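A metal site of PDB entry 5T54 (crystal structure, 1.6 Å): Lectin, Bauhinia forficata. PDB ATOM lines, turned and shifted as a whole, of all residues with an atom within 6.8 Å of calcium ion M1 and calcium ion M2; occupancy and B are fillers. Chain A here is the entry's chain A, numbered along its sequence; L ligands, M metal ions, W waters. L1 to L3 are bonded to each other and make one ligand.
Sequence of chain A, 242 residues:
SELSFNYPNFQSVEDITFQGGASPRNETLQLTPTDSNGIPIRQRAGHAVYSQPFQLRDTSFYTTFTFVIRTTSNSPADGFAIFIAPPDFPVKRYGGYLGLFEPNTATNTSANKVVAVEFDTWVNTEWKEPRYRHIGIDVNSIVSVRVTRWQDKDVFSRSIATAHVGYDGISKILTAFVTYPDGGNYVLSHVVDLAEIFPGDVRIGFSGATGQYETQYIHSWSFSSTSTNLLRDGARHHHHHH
Of the 22 residues printed, 4 come within 4 Å of calcium ion M1.
An oxygen (O2) of LG3 L3 lies within hydrogen-bond range of the side-chain amide nitrogen of Asn 124, 2.8 Å away.
An oxygen (O1) of LIG L1 sits at hydrogen-bond distance from the indole nitrogen (NE1) of Trp 122 (3.0 Å).
O of Val 123 is in hydrogen-bond range of O2 of LIG L1, at 2.7 Å.
An oxygen (O5) of LG3 L3 is in hydrogen-bond range of the backbone NH of Gly 96 (2.9 Å).
The side-chain carboxylate (OD2) of Asp 78 is in hydrogen-bond range of an oxygen (O3) of LG3 L3.
Calcium ion M1 is bound by the side-chain amide oxygen (OD1) of Asn 124, the backbone carbonyl oxygen (O) of Trp 122, the side-chain carboxylate (OE2) of Glu 129, the side-chain carboxylate (OD2) of Asp 120, water W4, water W2 and the side-chain carboxylate (OD1) of Asp 120.
Along chain A the residues within 4 Å of calcium ion M2 span positions 118 to 134.
Water W1 bridges OE1 of Glu 118 and O of Ile 142.
OD2 of Asp 138 lies close to OE1 of Glu 118, at 2.5 Å.
The backbone NH of Glu 118 sits at hydrogen-bond distance from the backbone carbonyl oxygen of Gly 136.
The indole nitrogen of Trp 127 lies close to the side-chain carboxylate of Glu 129 (3.0 Å).
Calcium ion M2 is bound by OE2 of Glu 118 (2.2 Å), OD2 of Asp 120 (2.2 Å), water W1 (2.3 Å), water W3 (2.3 Å), OE1 of Glu 129 (2.3 Å) and NE2 of His 134 (2.4 Å).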
ATOM      1  N   ASP A  78      -5.633  18.821 -21.279  1.00  0.00           N
ATOM      2  CA  ASP A  78      -5.730  18.846 -22.754  1.00  0.00           C
ATOM      3  C   ASP A  78      -4.509  19.444 -23.448  1.00  0.00           C
ATOM      4  O   ASP A  78      -4.365  19.290 -24.692  1.00  0.00           O
ATOM      5  CB  ASP A  78      -6.965  19.643 -23.116  1.00  0.00           C
ATOM      6  CG  ASP A  78      -8.204  18.776 -23.074  1.00  0.00           C
ATOM      7  OD1 ASP A  78      -8.461  18.111 -24.103  1.00  0.00           O
ATOM      8  OD2 ASP A  78      -8.877  18.772 -21.969  1.00  0.00           O
ATOM      9  N   GLY A  95     -11.308  22.046 -21.724  1.00  0.00           N
ATOM     10  CA  GLY A  95     -11.249  20.819 -22.527  1.00  0.00           C
ATOM     11  C   GLY A  95     -10.422  21.037 -23.776  1.00  0.00           C
ATOM     12  O   GLY A  95      -9.444  21.795 -23.788  1.00  0.00           O
ATOM     13  N   GLY A  96     -10.805  20.343 -24.826  1.00  0.00           N
ATOM     14  CA  GLY A  96     -10.036  20.293 -26.081  1.00  0.00           C
ATOM     15  C   GLY A  96      -9.965  21.635 -26.797  1.00  0.00           C
ATOM     16  O   GLY A  96      -9.148  21.771 -27.721  1.00  0.00           O
ATOM     17  N   TYR A  97     -10.848  22.559 -26.452  1.00  0.00           N
ATOM     18  CA  TYR A  97     -10.813  23.908 -27.002  1.00  0.00           C
ATOM     19  C   TYR A  97      -9.583  24.698 -26.534  1.00  0.00           C
ATOM     20  O   TYR A  97      -9.363  25.828 -27.072  1.00  0.00           O
ATOM     21  CB  TYR A  97     -12.128  24.679 -26.704  1.00  0.00           C
ATOM     22  CG  TYR A  97     -13.306  23.880 -27.194  1.00  0.00           C
ATOM     23  CD1 TYR A  97     -13.579  23.800 -28.566  1.00  0.00           C
ATOM     24  CD2 TYR A  97     -14.083  23.157 -26.341  1.00  0.00           C
ATOM     25  CE1 TYR A  97     -14.625  22.977 -29.030  1.00  0.00           C
ATOM     26  CE2 TYR A  97     -15.114  22.317 -26.803  1.00  0.00           C
ATOM     27  CZ  TYR A  97     -15.385  22.266 -28.150  1.00  0.00           C
ATOM     28  OH  TYR A  97     -16.400  21.496 -28.660  1.00  0.00           O
ATOM     29  N   LEU A  98      -8.818  24.217 -25.529  1.00  0.00           N
ATOM     30  CA  LEU A  98      -7.548  24.815 -25.057  1.00  0.00           C
ATOM     31  C   LEU A  98      -7.660  26.235 -24.593  1.00  0.00           C
ATOM     32  O   LEU A  98      -6.679  26.987 -24.570  1.00  0.00           O
ATOM     33  CB  LEU A  98      -6.495  24.707 -26.227  1.00  0.00           C
ATOM     34  CG  LEU A  98      -6.112  23.277 -26.545  1.00  0.00           C
ATOM     35  CD1 LEU A  98      -5.148  23.214 -27.722  1.00  0.00           C
ATOM     36  CD2 LEU A  98      -5.538  22.589 -25.341  1.00  0.00           C
ATOM     37  N   GLU A 118       0.115  25.148 -30.572  1.00  0.00           N
ATOM     38  CA  GLU A 118      -0.454  24.270 -29.557  1.00  0.00           C
ATOM     39  C   GLU A 118       0.388  23.043 -29.247  1.00  0.00           C
ATOM     40  O   GLU A 118       1.083  22.499 -30.125  1.00  0.00           O
ATOM     41  CB  GLU A 118      -1.898  23.843 -29.948  1.00  0.00           C
ATOM     42  CG  GLU A 118      -2.037  23.002 -31.177  1.00  0.00           C
ATOM     43  CD  GLU A 118      -3.406  22.344 -31.268  1.00  0.00           C
ATOM     44  OE1 GLU A 118      -4.417  23.098 -31.305  1.00  0.00           O
ATOM     45  OE2 GLU A 118      -3.502  21.109 -31.470  1.00  0.00           O
ATOM     46  N   ASP A 120      -0.655  19.549 -27.734  1.00  0.00           N
ATOM     47  CA  ASP A 120      -1.973  18.917 -27.556  1.00  0.00           C
ATOM     48  C   ASP A 120      -1.776  17.498 -27.002  1.00  0.00           C
ATOM     49  O   ASP A 120      -1.221  16.610 -27.660  1.00  0.00           O
ATOM     50  CB  ASP A 120      -2.726  18.938 -28.874  1.00  0.00           C
ATOM     51  CG  ASP A 120      -4.128  18.491 -28.740  1.00  0.00           C
ATOM     52  OD1 ASP A 120      -4.415  17.719 -27.805  1.00  0.00           O
ATOM     53  OD2 ASP A 120      -5.007  18.878 -29.592  1.00  0.00           O
ATOM     54  N   THR A 121      -2.206  17.275 -25.730  1.00  0.00           N
ATOM     55  CA  THR A 121      -1.991  16.047 -25.028  1.00  0.00           C
ATOM     56  C   THR A 121      -3.151  15.076 -25.130  1.00  0.00           C
ATOM     57  O   THR A 121      -2.995  13.965 -24.620  1.00  0.00           O
ATOM     58  CB  THR A 121      -1.737  16.288 -23.529  1.00  0.00           C
ATOM     59  OG1 THR A 121      -2.885  17.016 -22.949  1.00  0.00           O
ATOM     60  CG2 THR A 121      -0.430  17.067 -23.290  1.00  0.00           C
ATOM     61  N   TRP A 122      -4.291  15.499 -25.663  1.00  0.00           N
ATOM     62  CA  TRP A 122      -5.491  14.636 -25.683  1.00  0.00           C
ATOM     63  C   TRP A 122      -6.033  14.579 -27.097  1.00  0.00           C
ATOM     64  O   TRP A 122      -6.448  15.638 -27.639  1.00  0.00           O
ATOM     65  CB  TRP A 122      -6.566  15.173 -24.739  1.00  0.00           C
ATOM     66  CG  TRP A 122      -7.842  14.382 -24.760  1.00  0.00           C
ATOM     67  CD1 TRP A 122      -8.816  14.580 -25.644  1.00  0.00           C
ATOM     68  CD2 TRP A 122      -8.255  13.291 -23.914  1.00  0.00           C
ATOM     69  NE1 TRP A 122      -9.848  13.676 -25.441  1.00  0.00           N
ATOM     70  CE2 TRP A 122      -9.523  12.895 -24.364  1.00  0.00           C
ATOM     71  CE3 TRP A 122      -7.636  12.585 -22.850  1.00  0.00           C
ATOM     72  CZ2 TRP A 122     -10.264  11.860 -23.763  1.00  0.00           C
ATOM     73  CZ3 TRP A 122      -8.368  11.566 -22.212  1.00  0.00           C
ATOM     74  CH2 TRP A 122      -9.656  11.210 -22.682  1.00  0.00           C
ATOM     75  N   VAL A 123      -6.053  13.385 -27.676  1.00  0.00           N
ATOM     76  CA  VAL A 123      -6.642  13.188 -28.968  1.00  0.00           C
ATOM     77  C   VAL A 123      -8.219  13.350 -28.939  1.00  0.00           C
ATOM     78  O   VAL A 123      -8.921  12.546 -28.344  1.00  0.00           O
ATOM     79  CB  VAL A 123      -6.256  11.819 -29.574  1.00  0.00           C
ATOM     80  CG1 VAL A 123      -7.009  11.538 -30.845  1.00  0.00           C
ATOM     81  CG2 VAL A 123      -4.750  11.750 -29.751  1.00  0.00           C
ATOM     82  N   ASN A 124      -8.709  14.409 -29.607  1.00  0.00           N
ATOM     83  CA  ASN A 124     -10.105  14.668 -29.742  1.00  0.00           C
ATOM     84  C   ASN A 124     -10.676  14.111 -31.035  1.00  0.00           C
ATOM     85  O   ASN A 124     -10.060  14.163 -32.105  1.00  0.00           O
ATOM     86  CB  ASN A 124     -10.363  16.161 -29.717  1.00  0.00           C
ATOM     87  CG  ASN A 124     -10.153  16.741 -28.360  1.00  0.00           C
ATOM     88  OD1 ASN A 124      -9.102  17.282 -28.092  1.00  0.00           O
ATOM     89  ND2 ASN A 124     -11.186  16.729 -27.518  1.00  0.00           N
ATOM     90  N   TRP A 127     -13.571  16.929 -33.525  1.00  0.00           N
ATOM     91  CA  TRP A 127     -13.137  17.631 -34.758  1.00  0.00           C
ATOM     92  C   TRP A 127     -11.939  16.841 -35.263  1.00  0.00           C
ATOM     93  O   TRP A 127     -11.417  15.909 -34.575  1.00  0.00           O
ATOM     94  CB  TRP A 127     -12.681  19.092 -34.460  1.00  0.00           C
ATOM     95  CG  TRP A 127     -11.754  19.195 -33.286  1.00  0.00           C
ATOM     96  CD1 TRP A 127     -10.353  19.091 -33.268  1.00  0.00           C
ATOM     97  CD2 TRP A 127     -12.121  19.477 -31.945  1.00  0.00           C
ATOM     98  NE1 TRP A 127      -9.890  19.246 -31.991  1.00  0.00           N
ATOM     99  CE2 TRP A 127     -10.955  19.511 -31.176  1.00  0.00           C
ATOM    100  CE3 TRP A 127     -13.366  19.704 -31.306  1.00  0.00           C
ATOM    101  CZ2 TRP A 127     -10.971  19.775 -29.829  1.00  0.00           C
ATOM    102  CZ3 TRP A 127     -13.336  19.945 -29.930  1.00  0.00           C
ATOM    103  CH2 TRP A 127     -12.180  19.989 -29.224  1.00  0.00           C
ATOM    104  N   LYS A 128     -11.480  17.176 -36.450  1.00  0.00           N
ATOM    105  CA  LYS A 128     -10.381  16.481 -37.116  1.00  0.00           C
ATOM    106  C   LYS A 128      -9.055  16.848 -36.427  1.00  0.00           C
ATOM    107  O   LYS A 128      -8.669  18.022 -36.430  1.00  0.00           O
ATOM    108  CB  LYS A 128     -10.292  16.910 -38.604  1.00  0.00           C
ATOM    109  CG  LYS A 128      -9.033  16.386 -39.295  1.00  0.00           C
ATOM    110  CD  LYS A 128      -9.104  16.465 -40.829  1.00  0.00           C
ATOM    111  CE  LYS A 128      -9.125  17.914 -41.383  1.00  0.00           C
ATOM    112  NZ  LYS A 128      -7.732  18.475 -41.560  1.00  0.00           N
ATOM    113  N   GLU A 129      -8.352  15.882 -35.895  1.00  0.00           N
ATOM    114  CA  GLU A 129      -6.926  16.070 -35.526  1.00  0.00           C
ATOM    115  C   GLU A 129      -6.254  14.715 -35.509  1.00  0.00           C
ATOM    116  O   GLU A 129      -6.978  13.655 -35.696  1.00  0.00           O
ATOM    117  CB  GLU A 129      -6.738  16.843 -34.200  1.00  0.00           C
ATOM    118  CG  GLU A 129      -7.296  16.168 -32.951  1.00  0.00           C
ATOM    119  CD  GLU A 129      -7.162  17.097 -31.688  1.00  0.00           C
ATOM    120  OE1 GLU A 129      -7.026  18.336 -31.851  1.00  0.00           O
ATOM    121  OE2 GLU A 129      -7.076  16.577 -30.554  1.00  0.00           O
ATOM    122  N   PRO A 130      -4.933  14.693 -35.452  1.00  0.00           N
ATOM    123  CA  PRO A 130      -4.255  13.380 -35.572  1.00  0.00           C
ATOM    124  C   PRO A 130      -4.591  12.423 -34.459  1.00  0.00           C
ATOM    125  O   PRO A 130      -5.003  12.836 -33.356  1.00  0.00           O
ATOM    126  CB  PRO A 130      -2.759  13.730 -35.498  1.00  0.00           C
ATOM    127  CG  PRO A 130      -2.680  15.158 -35.787  1.00  0.00           C
ATOM    128  CD  PRO A 130      -3.956  15.771 -35.288  1.00  0.00           C
ATOM    129  N   HIS A 134       0.286  15.714 -30.341  1.00  0.00           N
ATOM    130  CA  HIS A 134       0.769  16.483 -31.448  1.00  0.00           C
ATOM    131  C   HIS A 134       1.035  17.897 -31.044  1.00  0.00           C
ATOM    132  O   HIS A 134       0.457  18.429 -30.118  1.00  0.00           O
ATOM    133  CB  HIS A 134      -0.191  16.412 -32.676  1.00  0.00           C
ATOM    134  CG  HIS A 134      -1.618  16.785 -32.369  1.00  0.00           C
ATOM    135  ND1 HIS A 134      -2.525  15.874 -31.870  1.00  0.00           N
ATOM    136  CD2 HIS A 134      -2.272  17.957 -32.463  1.00  0.00           C
ATOM    137  CE1 HIS A 134      -3.685  16.485 -31.683  1.00  0.00           C
ATOM    138  NE2 HIS A 134      -3.551  17.738 -32.072  1.00  0.00           N
ATOM    139  N   GLY A 136       0.971  21.656 -33.051  1.00  0.00           N
ATOM    140  CA  GLY A 136       0.425  22.292 -34.224  1.00  0.00           C
ATOM    141  C   GLY A 136       0.472  23.789 -34.222  1.00  0.00           C
ATOM    142  O   GLY A 136       0.602  24.449 -33.181  1.00  0.00           O
ATOM    143  N   ASP A 138      -2.155  26.763 -35.300  1.00  0.00           N
ATOM    144  CA  ASP A 138      -3.653  27.044 -35.397  1.00  0.00           C
ATOM    145  C   ASP A 138      -3.833  28.412 -35.938  1.00  0.00           C
ATOM    146  O   ASP A 138      -3.210  29.372 -35.447  1.00  0.00           O
ATOM    147  CB  ASP A 138      -4.330  26.909 -34.033  1.00  0.00           C
ATOM    148  CG  ASP A 138      -4.186  25.553 -33.458  1.00  0.00           C
ATOM    149  OD1 ASP A 138      -3.908  24.582 -34.182  1.00  0.00           O
ATOM    150  OD2 ASP A 138      -4.439  25.411 -32.225  1.00  0.00           O
ATOM    151  N   ILE A 142      -9.491  25.382 -34.247  1.00  0.00           N
ATOM    152  CA  ILE A 142      -8.929  24.320 -33.444  1.00  0.00           C
ATOM    153  C   ILE A 142      -8.370  23.166 -34.317  1.00  0.00           C
ATOM    154  O   ILE A 142      -7.677  22.309 -33.806  1.00  0.00           O
ATOM    155  CB  ILE A 142      -9.993  23.849 -32.417  1.00  0.00           C
ATOM    156  CG1 ILE A 142      -9.395  23.118 -31.218  1.00  0.00           C
ATOM    157  CG2 ILE A 142     -11.073  23.006 -33.102  1.00  0.00           C
ATOM    158  CD1 ILE A 142      -8.376  23.823 -30.392  1.00  0.00           C
ATOM    159  N   VAL A 143      -8.704  23.114 -35.566  1.00  0.00           N
ATOM    160  CA  VAL A 143      -8.159  22.141 -36.554  1.00  0.00           C
ATOM    161  C   VAL A 143      -6.887  22.820 -37.091  1.00  0.00           C
ATOM    162  O   VAL A 143      -6.974  23.731 -37.923  1.00  0.00           O
ATOM    163  CB  VAL A 143      -9.192  21.835 -37.663  1.00  0.00           C
ATOM    164  CG1 VAL A 143      -8.610  20.849 -38.686  1.00  0.00           C
ATOM    165  CG2 VAL A 143     -10.415  21.180 -37.005  1.00  0.00           C
ATOM    166  N   SER A 144      -5.761  22.272 -36.701  1.00  0.00           N
ATOM    167  CA  SER A 144      -4.428  22.873 -36.968  1.00  0.00           C
ATOM    168  C   SER A 144      -4.150  22.868 -38.490  1.00  0.00           C
ATOM    169  O   SER A 144      -4.529  21.932 -39.200  1.00  0.00           O
ATOM    170  CB  SER A 144      -3.318  22.069 -36.315  1.00  0.00           C
ATOM    171  OG  SER A 144      -3.477  22.009 -34.900  1.00  0.00           O
ATOM    172  N   VAL A 147       0.576  20.312 -38.507  1.00  0.00           N
ATOM    173  CA  VAL A 147       0.567  19.498 -37.313  1.00  0.00           C
ATOM    174  C   VAL A 147       1.553  18.363 -37.408  1.00  0.00           C
ATOM    175  O   VAL A 147       1.718  17.766 -38.516  1.00  0.00           O
ATOM    176  CB  VAL A 147      -0.898  19.009 -37.086  1.00  0.00           C
ATOM    177  CG1 VAL A 147      -1.251  17.904 -38.080  1.00  0.00           C
ATOM    178  CG2 VAL A 147      -1.083  18.584 -35.675  1.00  0.00           C
HETATM  179  C1  LIG L   1     -14.238  12.065 -26.487  1.00  0.00           C
HETATM  180  C2  LIG L   1     -13.050  12.217 -27.429  1.00  0.00           C
HETATM  181  C3  LIG L   1     -12.136  10.999 -27.403  1.00  0.00           C
HETATM  182  C4  LIG L   1     -12.929   9.680 -27.601  1.00  0.00           C
HETATM  183  C5  LIG L   1     -14.035   9.723 -26.571  1.00  0.00           C
HETATM  184  C6  LIG L   1     -14.844   8.408 -26.557  1.00  0.00           C
HETATM  185  O1  LIG L   1     -12.380  13.467 -27.110  1.00  0.00           O
HETATM  186  O2  LIG L   1     -11.245  11.143 -28.501  1.00  0.00           O
HETATM  187  O3  LIG L   1     -13.366   9.655 -28.944  1.00  0.00           O
HETATM  188  O4  LIG L   1     -14.890  10.828 -26.840  1.00  0.00           O
HETATM  189  C1  LG2 L   2     -15.633  11.204 -23.740  1.00  0.00           C
HETATM  190  C2  LG2 L   2     -15.006  12.434 -24.326  1.00  0.00           C
HETATM  191  C3  LG2 L   2     -14.550  13.347 -23.220  1.00  0.00           C
HETATM  192  C4  LG2 L   2     -15.645  13.548 -22.204  1.00  0.00           C
HETATM  193  C5  LG2 L   2     -16.243  12.274 -21.669  1.00  0.00           C
HETATM  194  C6  LG2 L   2     -17.469  12.575 -20.783  1.00  0.00           C
HETATM  195  O1  LG2 L   2     -14.600  10.500 -23.077  1.00  0.00           O
HETATM  196  O2  LG2 L   2     -13.844  12.121 -25.107  1.00  0.00           O
HETATM  197  O3  LG2 L   2     -14.040  14.602 -23.763  1.00  0.00           O
HETATM  198  O4  LG2 L   2     -16.640  14.260 -22.892  1.00  0.00           O
HETATM  199  O5  LG2 L   2     -16.688  11.512 -22.805  1.00  0.00           O
HETATM  200  O6  LG2 L   2     -17.770  11.280 -20.213  1.00  0.00           O
HETATM  201  O1  LG3 L   3     -12.981  15.306 -21.776  1.00  0.00           O
HETATM  202  C1  LG3 L   3     -13.724  15.686 -22.931  1.00  0.00           C
HETATM  203  C2  LG3 L   3     -13.014  16.739 -23.773  1.00  0.00           C
HETATM  204  N1  LG3 L   3     -13.832  17.024 -24.911  1.00  0.00           N
HETATM  205  C3  LG3 L   3     -11.619  16.290 -24.080  1.00  0.00           C
HETATM  206  O2  LG3 L   3     -10.983  17.382 -24.765  1.00  0.00           O
HETATM  207  C4  LG3 L   3     -10.920  15.916 -22.764  1.00  0.00           C
HETATM  208  O3  LG3 L   3     -10.753  17.001 -21.832  1.00  0.00           O
HETATM  209  C5  LG3 L   3     -11.700  14.778 -22.104  1.00  0.00           C
HETATM  210  C6  LG3 L   3     -11.042  14.318 -20.810  1.00  0.00           C
HETATM  211  O4  LG3 L   3     -11.825  13.208 -20.286  1.00  0.00           O
HETATM  212  C7  LG3 L   3     -13.990  18.251 -25.364  1.00  0.00           C
HETATM  213  O5  LG3 L   3     -13.519  19.235 -24.777  1.00  0.00           O
HETATM  214  C8  LG3 L   3     -14.734  18.413 -26.668  1.00  0.00           C
HETATM  215 CA    CA M   1      -6.873  17.785 -28.497  1.00  0.00          CA
HETATM  216 CA    CA M   2      -5.045  19.569 -31.723  1.00  0.00          CA
HETATM  217  O   HOH W   1      -6.429  21.341 -31.469  1.00  0.00           O
HETATM  218  O   HOH W   2      -7.716  19.974 -29.170  1.00  0.00           O
HETATM  219  O   HOH W   3      -4.743  19.942 -33.975  1.00  0.00           O
HETATM  220  O   HOH W   4      -6.851  18.555 -26.197  1.00  0.00           O
